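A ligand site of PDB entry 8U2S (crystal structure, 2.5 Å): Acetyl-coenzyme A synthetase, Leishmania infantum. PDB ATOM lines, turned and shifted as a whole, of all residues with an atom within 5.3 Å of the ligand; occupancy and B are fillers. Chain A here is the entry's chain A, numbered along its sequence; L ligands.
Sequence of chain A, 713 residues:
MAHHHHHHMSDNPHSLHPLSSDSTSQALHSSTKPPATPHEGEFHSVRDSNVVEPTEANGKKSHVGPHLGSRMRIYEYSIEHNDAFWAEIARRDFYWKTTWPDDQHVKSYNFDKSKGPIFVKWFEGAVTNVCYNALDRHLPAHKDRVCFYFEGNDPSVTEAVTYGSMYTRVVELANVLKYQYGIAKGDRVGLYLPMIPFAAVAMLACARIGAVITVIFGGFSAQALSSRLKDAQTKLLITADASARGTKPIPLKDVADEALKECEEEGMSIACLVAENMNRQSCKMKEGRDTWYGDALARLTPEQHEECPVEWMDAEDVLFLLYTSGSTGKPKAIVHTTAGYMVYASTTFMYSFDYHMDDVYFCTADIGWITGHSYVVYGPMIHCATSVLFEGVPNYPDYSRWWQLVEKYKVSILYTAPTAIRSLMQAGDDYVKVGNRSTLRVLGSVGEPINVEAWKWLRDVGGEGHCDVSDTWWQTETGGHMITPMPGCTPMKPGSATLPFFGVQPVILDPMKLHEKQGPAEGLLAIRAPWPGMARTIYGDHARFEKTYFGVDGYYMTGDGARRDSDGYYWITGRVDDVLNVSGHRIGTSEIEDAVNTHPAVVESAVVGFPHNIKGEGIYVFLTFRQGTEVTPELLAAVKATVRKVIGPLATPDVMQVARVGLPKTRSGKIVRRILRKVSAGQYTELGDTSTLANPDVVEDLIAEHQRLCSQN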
ATOM      1  N   THR A 324      -7.420  -0.492  37.808  1.00  0.00           N
ATOM      2  CA  THR A 324      -6.041  -0.748  37.432  1.00  0.00           C
ATOM      3  C   THR A 324      -5.110   0.074  38.310  1.00  0.00           C
ATOM      4  O   THR A 324      -5.376   1.258  38.558  1.00  0.00           O
ATOM      5  CB  THR A 324      -5.798  -0.414  35.960  1.00  0.00           C
ATOM      6  OG1 THR A 324      -6.814  -1.034  35.161  1.00  0.00           O
ATOM      7  CG2 THR A 324      -4.433  -0.899  35.510  1.00  0.00           C
ATOM      8  N   ILE A 370      -7.391  -7.739  32.465  1.00  0.00           N
ATOM      9  CA  ILE A 370      -7.747  -7.371  31.102  1.00  0.00           C
ATOM     10  C   ILE A 370      -7.505  -8.530  30.153  1.00  0.00           C
ATOM     11  O   ILE A 370      -8.212  -8.687  29.153  1.00  0.00           O
ATOM     12  CB  ILE A 370      -6.958  -6.121  30.652  1.00  0.00           C
ATOM     13  CG1 ILE A 370      -7.452  -5.642  29.286  1.00  0.00           C
ATOM     14  CG2 ILE A 370      -5.456  -6.405  30.604  1.00  0.00           C
ATOM     15  CD1 ILE A 370      -8.868  -5.109  29.305  1.00  0.00           C
ATOM     16  N   THR A 371      -6.500  -9.376  30.445  1.00  0.00           N
ATOM     17  CA  THR A 371      -6.217 -10.506  29.562  1.00  0.00           C
ATOM     18  C   THR A 371      -7.415 -11.436  29.466  1.00  0.00           C
ATOM     19  O   THR A 371      -7.685 -12.012  28.411  1.00  0.00           O
ATOM     20  CB  THR A 371      -4.990 -11.271  30.073  1.00  0.00           C
ATOM     21  OG1 THR A 371      -3.869 -10.384  30.135  1.00  0.00           O
ATOM     22  CG2 THR A 371      -4.663 -12.438  29.144  1.00  0.00           C
ATOM     23  N   SER A 445       2.844 -15.368  25.255  1.00  0.00           N
ATOM     24  CA  SER A 445       3.334 -14.843  26.527  1.00  0.00           C
ATOM     25  C   SER A 445       2.795 -13.434  26.712  1.00  0.00           C
ATOM     26  O   SER A 445       2.733 -12.649  25.760  1.00  0.00           O
ATOM     27  CB  SER A 445       4.863 -14.836  26.569  1.00  0.00           C
ATOM     28  OG  SER A 445       5.342 -14.593  27.873  1.00  0.00           O
ATOM     29  N   VAL A 446       2.395 -13.116  27.945  1.00  0.00           N
ATOM     30  CA  VAL A 446       1.793 -11.825  28.241  1.00  0.00           C
ATOM     31  C   VAL A 446       2.048 -11.477  29.698  1.00  0.00           C
ATOM     32  O   VAL A 446       2.223 -12.370  30.546  1.00  0.00           O
ATOM     33  CB  VAL A 446       0.272 -11.824  27.938  1.00  0.00           C
ATOM     34  CG1 VAL A 446      -0.394 -13.002  28.617  1.00  0.00           C
ATOM     35  CG2 VAL A 446      -0.359 -10.517  28.382  1.00  0.00           C
ATOM     36  N   GLY A 447       2.087 -10.176  29.986  1.00  0.00           N
ATOM     37  CA  GLY A 447       2.065  -9.664  31.337  1.00  0.00           C
ATOM     38  C   GLY A 447       3.375  -9.029  31.780  1.00  0.00           C
ATOM     39  O   GLY A 447       3.361  -8.101  32.596  1.00  0.00           O
ATOM     40  N   GLU A 448       4.497  -9.512  31.259  1.00  0.00           N
ATOM     41  CA  GLU A 448       5.795  -9.043  31.705  1.00  0.00           C
ATOM     42  C   GLU A 448       6.874  -9.590  30.772  1.00  0.00           C
ATOM     43  O   GLU A 448       6.584 -10.465  29.953  1.00  0.00           O
ATOM     44  CB  GLU A 448       6.040  -9.469  33.160  1.00  0.00           C
ATOM     45  CG  GLU A 448       6.173 -10.966  33.388  1.00  0.00           C
ATOM     46  CD  GLU A 448       6.502 -11.298  34.845  1.00  0.00           C
ATOM     47  OE1 GLU A 448       6.124 -10.520  35.739  1.00  0.00           O
ATOM     48  OE2 GLU A 448       7.139 -12.349  35.084  1.00  0.00           O
ATOM     49  N   PRO A 449       8.102  -9.086  30.849  1.00  0.00           N
ATOM     50  CA  PRO A 449       9.146  -9.585  29.944  1.00  0.00           C
ATOM     51  C   PRO A 449       9.412 -11.058  30.166  1.00  0.00           C
ATOM     52  O   PRO A 449       9.303 -11.568  31.289  1.00  0.00           O
ATOM     53  CB  PRO A 449      10.370  -8.734  30.308  1.00  0.00           C
ATOM     54  CG  PRO A 449       9.856  -7.591  31.133  1.00  0.00           C
ATOM     55  CD  PRO A 449       8.632  -8.102  31.812  1.00  0.00           C
ATOM     56  N   ASP A 471       4.937 -13.265  21.842  1.00  0.00           N
ATOM     57  CA  ASP A 471       5.141 -12.431  23.027  1.00  0.00           C
ATOM     58  C   ASP A 471       4.447 -11.090  22.783  1.00  0.00           C
ATOM     59  O   ASP A 471       4.986 -10.219  22.110  1.00  0.00           O
ATOM     60  CB  ASP A 471       6.631 -12.240  23.298  1.00  0.00           C
ATOM     61  CG  ASP A 471       6.912 -11.240  24.400  1.00  0.00           C
ATOM     62  OD1 ASP A 471       5.968 -10.859  25.123  1.00  0.00           O
ATOM     63  OD2 ASP A 471       8.094 -10.838  24.542  1.00  0.00           O
ATOM     64  N   THR A 472       3.255 -10.940  23.339  1.00  0.00           N
ATOM     65  CA  THR A 472       2.408  -9.777  23.085  1.00  0.00           C
ATOM     66  C   THR A 472       2.585  -8.745  24.198  1.00  0.00           C
ATOM     67  O   THR A 472       2.418  -9.072  25.375  1.00  0.00           O
ATOM     68  CB  THR A 472       0.945 -10.181  22.980  1.00  0.00           C
ATOM     69  OG1 THR A 472       0.505 -10.763  24.215  1.00  0.00           O
ATOM     70  CG2 THR A 472       0.746 -11.188  21.852  1.00  0.00           C
ATOM     71  N   TRP A 473       2.913  -7.516  23.815  1.00  0.00           N
ATOM     72  CA  TRP A 473       2.919  -6.401  24.750  1.00  0.00           C
ATOM     73  C   TRP A 473       1.662  -5.563  24.568  1.00  0.00           C
ATOM     74  O   TRP A 473       1.251  -5.274  23.443  1.00  0.00           O
ATOM     75  CB  TRP A 473       4.153  -5.507  24.578  1.00  0.00           C
ATOM     76  CG  TRP A 473       4.076  -4.322  25.489  1.00  0.00           C
ATOM     77  CD1 TRP A 473       4.524  -4.245  26.765  1.00  0.00           C
ATOM     78  CD2 TRP A 473       3.473  -3.055  25.183  1.00  0.00           C
ATOM     79  NE1 TRP A 473       4.248  -2.999  27.281  1.00  0.00           N
ATOM     80  CE2 TRP A 473       3.604  -2.250  26.333  1.00  0.00           C
ATOM     81  CE3 TRP A 473       2.845  -2.527  24.057  1.00  0.00           C
ATOM     82  CZ2 TRP A 473       3.137  -0.946  26.386  1.00  0.00           C
ATOM     83  CZ3 TRP A 473       2.378  -1.222  24.110  1.00  0.00           C
ATOM     84  CH2 TRP A 473       2.526  -0.449  25.270  1.00  0.00           C
ATOM     85  N   TRP A 474       1.078  -5.147  25.691  1.00  0.00           N
ATOM     86  CA  TRP A 474      -0.105  -4.285  25.695  1.00  0.00           C
ATOM     87  C   TRP A 474      -0.486  -3.981  27.134  1.00  0.00           C
ATOM     88  O   TRP A 474       0.242  -4.348  28.073  1.00  0.00           O
ATOM     89  CB  TRP A 474      -1.264  -4.947  24.943  1.00  0.00           C
ATOM     90  CG  TRP A 474      -1.704  -6.270  25.483  1.00  0.00           C
ATOM     91  CD1 TRP A 474      -0.969  -7.415  25.539  1.00  0.00           C
ATOM     92  CD2 TRP A 474      -2.992  -6.590  26.035  1.00  0.00           C
ATOM     93  NE1 TRP A 474      -1.720  -8.425  26.096  1.00  0.00           N
ATOM     94  CE2 TRP A 474      -2.958  -7.946  26.408  1.00  0.00           C
ATOM     95  CE3 TRP A 474      -4.168  -5.861  26.257  1.00  0.00           C
ATOM     96  CZ2 TRP A 474      -4.053  -8.587  26.985  1.00  0.00           C
ATOM     97  CZ3 TRP A 474      -5.249  -6.492  26.829  1.00  0.00           C
ATOM     98  CH2 TRP A 474      -5.185  -7.847  27.187  1.00  0.00           C
ATOM     99  N   GLN A 475      -1.620  -3.303  27.340  1.00  0.00           N
ATOM    100  CA  GLN A 475      -1.987  -2.812  28.658  1.00  0.00           C
ATOM    101  C   GLN A 475      -3.500  -2.863  28.801  1.00  0.00           C
ATOM    102  O   GLN A 475      -4.241  -2.988  27.825  1.00  0.00           O
ATOM    103  CB  GLN A 475      -1.519  -1.381  28.887  1.00  0.00           C
ATOM    104  CG  GLN A 475      -0.063  -1.112  28.587  1.00  0.00           C
ATOM    105  CD  GLN A 475       0.305   0.332  28.788  1.00  0.00           C
ATOM    106  OE1 GLN A 475      -0.347   1.231  28.248  1.00  0.00           O
ATOM    107  NE2 GLN A 475       1.336   0.579  29.587  1.00  0.00           N
ATOM    108  N   THR A 476      -3.959  -2.751  30.051  1.00  0.00           N
ATOM    109  CA  THR A 476      -5.384  -2.553  30.292  1.00  0.00           C
ATOM    110  C   THR A 476      -5.918  -1.379  29.487  1.00  0.00           C
ATOM    111  O   THR A 476      -7.042  -1.438  28.970  1.00  0.00           O
ATOM    112  CB  THR A 476      -5.635  -2.323  31.794  1.00  0.00           C
ATOM    113  OG1 THR A 476      -5.224  -3.481  32.529  1.00  0.00           O
ATOM    114  CG2 THR A 476      -7.112  -2.047  32.054  1.00  0.00           C
ATOM    115  N   GLU A 477      -5.117  -0.324  29.351  1.00  0.00           N
ATOM    116  CA  GLU A 477      -5.569   0.893  28.690  1.00  0.00           C
ATOM    117  C   GLU A 477      -5.625   0.756  27.171  1.00  0.00           C
ATOM    118  O   GLU A 477      -6.309   1.559  26.529  1.00  0.00           O
ATOM    119  CB  GLU A 477      -4.653   2.065  29.047  1.00  0.00           C
ATOM    120  CG  GLU A 477      -4.637   2.445  30.519  1.00  0.00           C
ATOM    121  CD  GLU A 477      -3.553   1.718  31.305  1.00  0.00           C
ATOM    122  OE1 GLU A 477      -3.186   0.587  30.912  1.00  0.00           O
ATOM    123  OE2 GLU A 477      -3.071   2.273  32.312  1.00  0.00           O
ATOM    124  N   THR A 558       2.755   5.277  27.671  1.00  0.00           N
ATOM    125  CA  THR A 558       2.443   3.933  28.149  1.00  0.00           C
ATOM    126  C   THR A 558       2.915   3.691  29.586  1.00  0.00           C
ATOM    127  O   THR A 558       2.370   2.807  30.259  1.00  0.00           O
ATOM    128  CB  THR A 558       3.078   2.867  27.256  1.00  0.00           C
ATOM    129  OG1 THR A 558       4.503   2.908  27.390  1.00  0.00           O
ATOM    130  CG2 THR A 558       2.708   3.109  25.800  1.00  0.00           C
ATOM    131  N   ASP A 560       5.840   2.528  30.126  1.00  0.00           N
ATOM    132  CA  ASP A 560       6.915   1.559  29.944  1.00  0.00           C
ATOM    133  C   ASP A 560       8.118   2.211  29.266  1.00  0.00           C
ATOM    134  O   ASP A 560       8.007   3.240  28.585  1.00  0.00           O
ATOM    135  CB  ASP A 560       6.443   0.378  29.102  1.00  0.00           C
ATOM    136  CG  ASP A 560       5.517  -0.548  29.845  1.00  0.00           C
ATOM    137  OD1 ASP A 560       5.878  -0.970  30.968  1.00  0.00           O
ATOM    138  OD2 ASP A 560       4.425  -0.856  29.323  1.00  0.00           O
ATOM    139  N   ILE A 572      10.637  -4.384  25.339  1.00  0.00           N
ATOM    140  CA  ILE A 572      10.063  -3.631  26.448  1.00  0.00           C
ATOM    141  C   ILE A 572      10.868  -3.911  27.715  1.00  0.00           C
ATOM    142  O   ILE A 572      11.054  -5.072  28.103  1.00  0.00           O
ATOM    143  CB  ILE A 572       8.584  -3.992  26.635  1.00  0.00           C
ATOM    144  CG1 ILE A 572       7.730  -3.305  25.554  1.00  0.00           C
ATOM    145  CG2 ILE A 572       8.099  -3.602  28.024  1.00  0.00           C
ATOM    146  CD1 ILE A 572       7.756  -4.005  24.209  1.00  0.00           C
ATOM    147  N   GLY A 574      10.244  -2.568  30.877  1.00  0.00           N
ATOM    148  CA  GLY A 574       9.473  -2.524  32.101  1.00  0.00           C
ATOM    149  C   GLY A 574       9.026  -1.116  32.441  1.00  0.00           C
ATOM    150  O   GLY A 574       9.338  -0.149  31.735  1.00  0.00           O
ATOM    151  N   ARG A 575       8.296  -1.014  33.544  1.00  0.00           N
ATOM    152  CA  ARG A 575       7.748   0.277  33.951  1.00  0.00           C
ATOM    153  C   ARG A 575       8.866   1.270  34.238  1.00  0.00           C
ATOM    154  O   ARG A 575       9.959   0.916  34.689  1.00  0.00           O
ATOM    155  CB  ARG A 575       6.873   0.121  35.200  1.00  0.00           C
ATOM    156  CG  ARG A 575       5.697  -0.836  35.039  1.00  0.00           C
ATOM    157  CD  ARG A 575       4.725  -0.398  33.955  1.00  0.00           C
ATOM    158  NE  ARG A 575       4.004   0.824  34.297  1.00  0.00           N
ATOM    159  CZ  ARG A 575       2.855   1.203  33.734  1.00  0.00           C
ATOM    160  NH1 ARG A 575       2.262   0.458  32.814  1.00  0.00           N
ATOM    161  NH2 ARG A 575       2.295   2.344  34.113  1.00  0.00           N
ATOM    162  N   ASN A 581       5.505  -5.037  38.630  1.00  0.00           N
ATOM    163  CA  ASN A 581       4.999  -6.200  37.906  1.00  0.00           C
ATOM    164  C   ASN A 581       5.412  -7.436  38.703  1.00  0.00           C
ATOM    165  O   ASN A 581       6.484  -7.993  38.490  1.00  0.00           O
ATOM    166  CB  ASN A 581       5.524  -6.244  36.483  1.00  0.00           C
ATOM    167  CG  ASN A 581       4.417  -6.218  35.451  1.00  0.00           C
ATOM    168  OD1 ASN A 581       3.873  -7.250  35.082  1.00  0.00           O
ATOM    169  ND2 ASN A 581       4.054  -5.015  35.009  1.00  0.00           N
ATOM    170  N   GLY A 584       3.386 -11.205  37.172  1.00  0.00           N
ATOM    171  CA  GLY A 584       2.522 -10.832  36.068  1.00  0.00           C
ATOM    172  C   GLY A 584       1.329  -9.976  36.432  1.00  0.00           C
ATOM    173  O   GLY A 584       0.482  -9.718  35.568  1.00  0.00           O
ATOM    174  N   ARG A 586      -0.199  -6.291  37.905  1.00  0.00           N
ATOM    175  CA  ARG A 586       0.153  -4.880  38.002  1.00  0.00           C
ATOM    176  C   ARG A 586      -0.271  -4.354  39.365  1.00  0.00           C
ATOM    177  O   ARG A 586      -1.451  -4.430  39.721  1.00  0.00           O
ATOM    178  CB  ARG A 586      -0.516  -4.075  36.885  1.00  0.00           C
ATOM    179  CG  ARG A 586       0.255  -2.815  36.543  1.00  0.00           C
ATOM    180  CD  ARG A 586      -0.645  -1.621  36.282  1.00  0.00           C
ATOM    181  NE  ARG A 586      -1.173  -1.609  34.929  1.00  0.00           N
ATOM    182  CZ  ARG A 586      -1.512  -0.514  34.258  1.00  0.00           C
ATOM    183  NH1 ARG A 586      -1.364   0.694  34.794  1.00  0.00           N
ATOM    184  NH2 ARG A 586      -1.988  -0.624  33.021  1.00  0.00           N
HETATM  185  C1  LIG L   1       3.695  -5.113  31.349  1.00  0.00           C
HETATM  186  C2  LIG L   1      -1.621  -6.827  31.014  1.00  0.00           C
HETATM  187  C3  LIG L   1       6.777  -6.851  28.801  1.00  0.00           C
HETATM  188  C4  LIG L   1       4.025  -3.676  30.954  1.00  0.00           C
HETATM  189  C5  LIG L   1      -1.747  -7.188  29.553  1.00  0.00           C
HETATM  190  C6  LIG L   1       2.637  -3.072  30.820  1.00  0.00           C
HETATM  191  C7  LIG L   1       4.712  -6.478  29.470  1.00  0.00           C
HETATM  192  C8  LIG L   1       1.839  -3.796  31.907  1.00  0.00           C
HETATM  193  C9  LIG L   1       4.181  -7.284  28.473  1.00  0.00           C
HETATM  194  C10 LIG L   1       0.354  -3.904  31.643  1.00  0.00           C
HETATM  195  C11 LIG L   1       5.104  -7.891  27.597  1.00  0.00           C
HETATM  196  C12 LIG L   1       2.534  -6.552  29.573  1.00  0.00           C
HETATM  197  N1  LIG L   1       6.411  -7.647  27.796  1.00  0.00           N
HETATM  198  N2  LIG L   1       6.010  -6.238  29.679  1.00  0.00           N
HETATM  199  N3  LIG L   1       4.730  -8.683  26.597  1.00  0.00           N
HETATM  200  N4  LIG L   1       2.821  -7.305  28.552  1.00  0.00           N
HETATM  201  N5  LIG L   1       3.640  -6.015  30.171  1.00  0.00           N
HETATM  202  O1  LIG L   1      -2.578  -3.433  32.635  1.00  0.00           O
HETATM  203  O2  LIG L   1       4.733  -3.074  32.027  1.00  0.00           O
HETATM  204  O3  LIG L   1      -2.285  -5.784  33.678  1.00  0.00           O
HETATM  205  O4  LIG L   1       2.607  -1.664  30.973  1.00  0.00           O
HETATM  206  O5  LIG L   1      -2.075  -5.497  31.195  1.00  0.00           O
HETATM  207  O6  LIG L   1       2.434  -5.117  31.972  1.00  0.00           O
HETATM  208  O7  LIG L   1      -0.328  -4.548  32.713  1.00  0.00           O
HETATM  209  P1  LIG L   1      -1.906  -4.767  32.650  1.00  0.00           P
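Merely in contact with the ligand: Ile 370 (3.6 Å), Thr 371 (3.9 Å), Val 446 (3.8 Å), Glu 448 (3.4 Å), Pro 449 (3.3 Å), Trp 473 (3.4 Å), Trp 474 (3.5 Å) and Ile 572 (3.6 Å).
Of the 23 residues printed, 17 come within 4 Å of the ligand.
The nearest printed residue that does not touch the ligand is Thr 324 (4.3 Å).
The side-chain carboxylate (OD2) of Asp 560 lies within hydrogen-bond range of the side-chain amide nitrogen (NE2) of Gln 475 (3.4 Å).
The side-chain hydroxyl (OG1) of Thr 558 is in hydrogen-bond range of the backbone NH (N) of Asp 560 (3.1 Å).
The backbone NH (N) of Thr 472 is in hydrogen-bond range of the backbone carbonyl oxygen (O) of Ser 445.
NH1 of Arg 575 sits at hydrogen-bond distance from O of Thr 558, at 3.5 Å.
NH2 of Arg 586 lies within salt-bridge range of OE1 of Glu 477 (2.7 Å).
The backbone carbonyl oxygen of Thr 558 lies within hydrogen-bond range of the side-chain amide nitrogen of Gln 475 (2.5 Å).
The backbone carbonyl oxygen (O) of Gly 447 sits close to the side-chain amide oxygen (OD1) of Asn 581 (2.7 Å).
The side-chain carboxylate of Glu 448 sits at hydrogen-bond distance from the backbone NH of Gly 584, 3.2 Å away.
The side-chain carboxylate (OD2) of Asp 560 sits at hydrogen-bond distance from an oxygen (O4) of the ligand (2.6 Å).
O of Thr 472 is in hydrogen-bond range of N3 of the ligand (2.6 Å).
The backbone NH of Thr 476 lies within hydrogen-bond range of an oxygen (O1) of the ligand (3.0 Å).
The side-chain hydroxyl of Thr 476 is in hydrogen-bond range of an oxygen (O1) of the ligand, 2.6 Å away.
NH1 of Arg 575 lies within hydrogen-bond range of O4 of the ligand, at 2.8 Å.
The guanidinium group (NH2) of Arg 586 is in salt-bridge range of an oxygen (O1) of the ligand.
The side-chain carboxylate (OD1) of Asp 471 lies within hydrogen-bond range of a nitrogen (N3) of the ligand (2.9 Å).
The side-chain amide nitrogen (NE2) of Gln 475 is in hydrogen-bond range of an oxygen (O4) of the ligand (2.9 Å).
A nitrogen (N4) of the ligand is in hydrogen-bond range of the backbone NH of Gly 447 (3.3 Å).
The side-chain amide nitrogen (ND2) of Asn 581 is in hydrogen-bond range of an oxygen (O6) of the ligand (3.4 Å).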
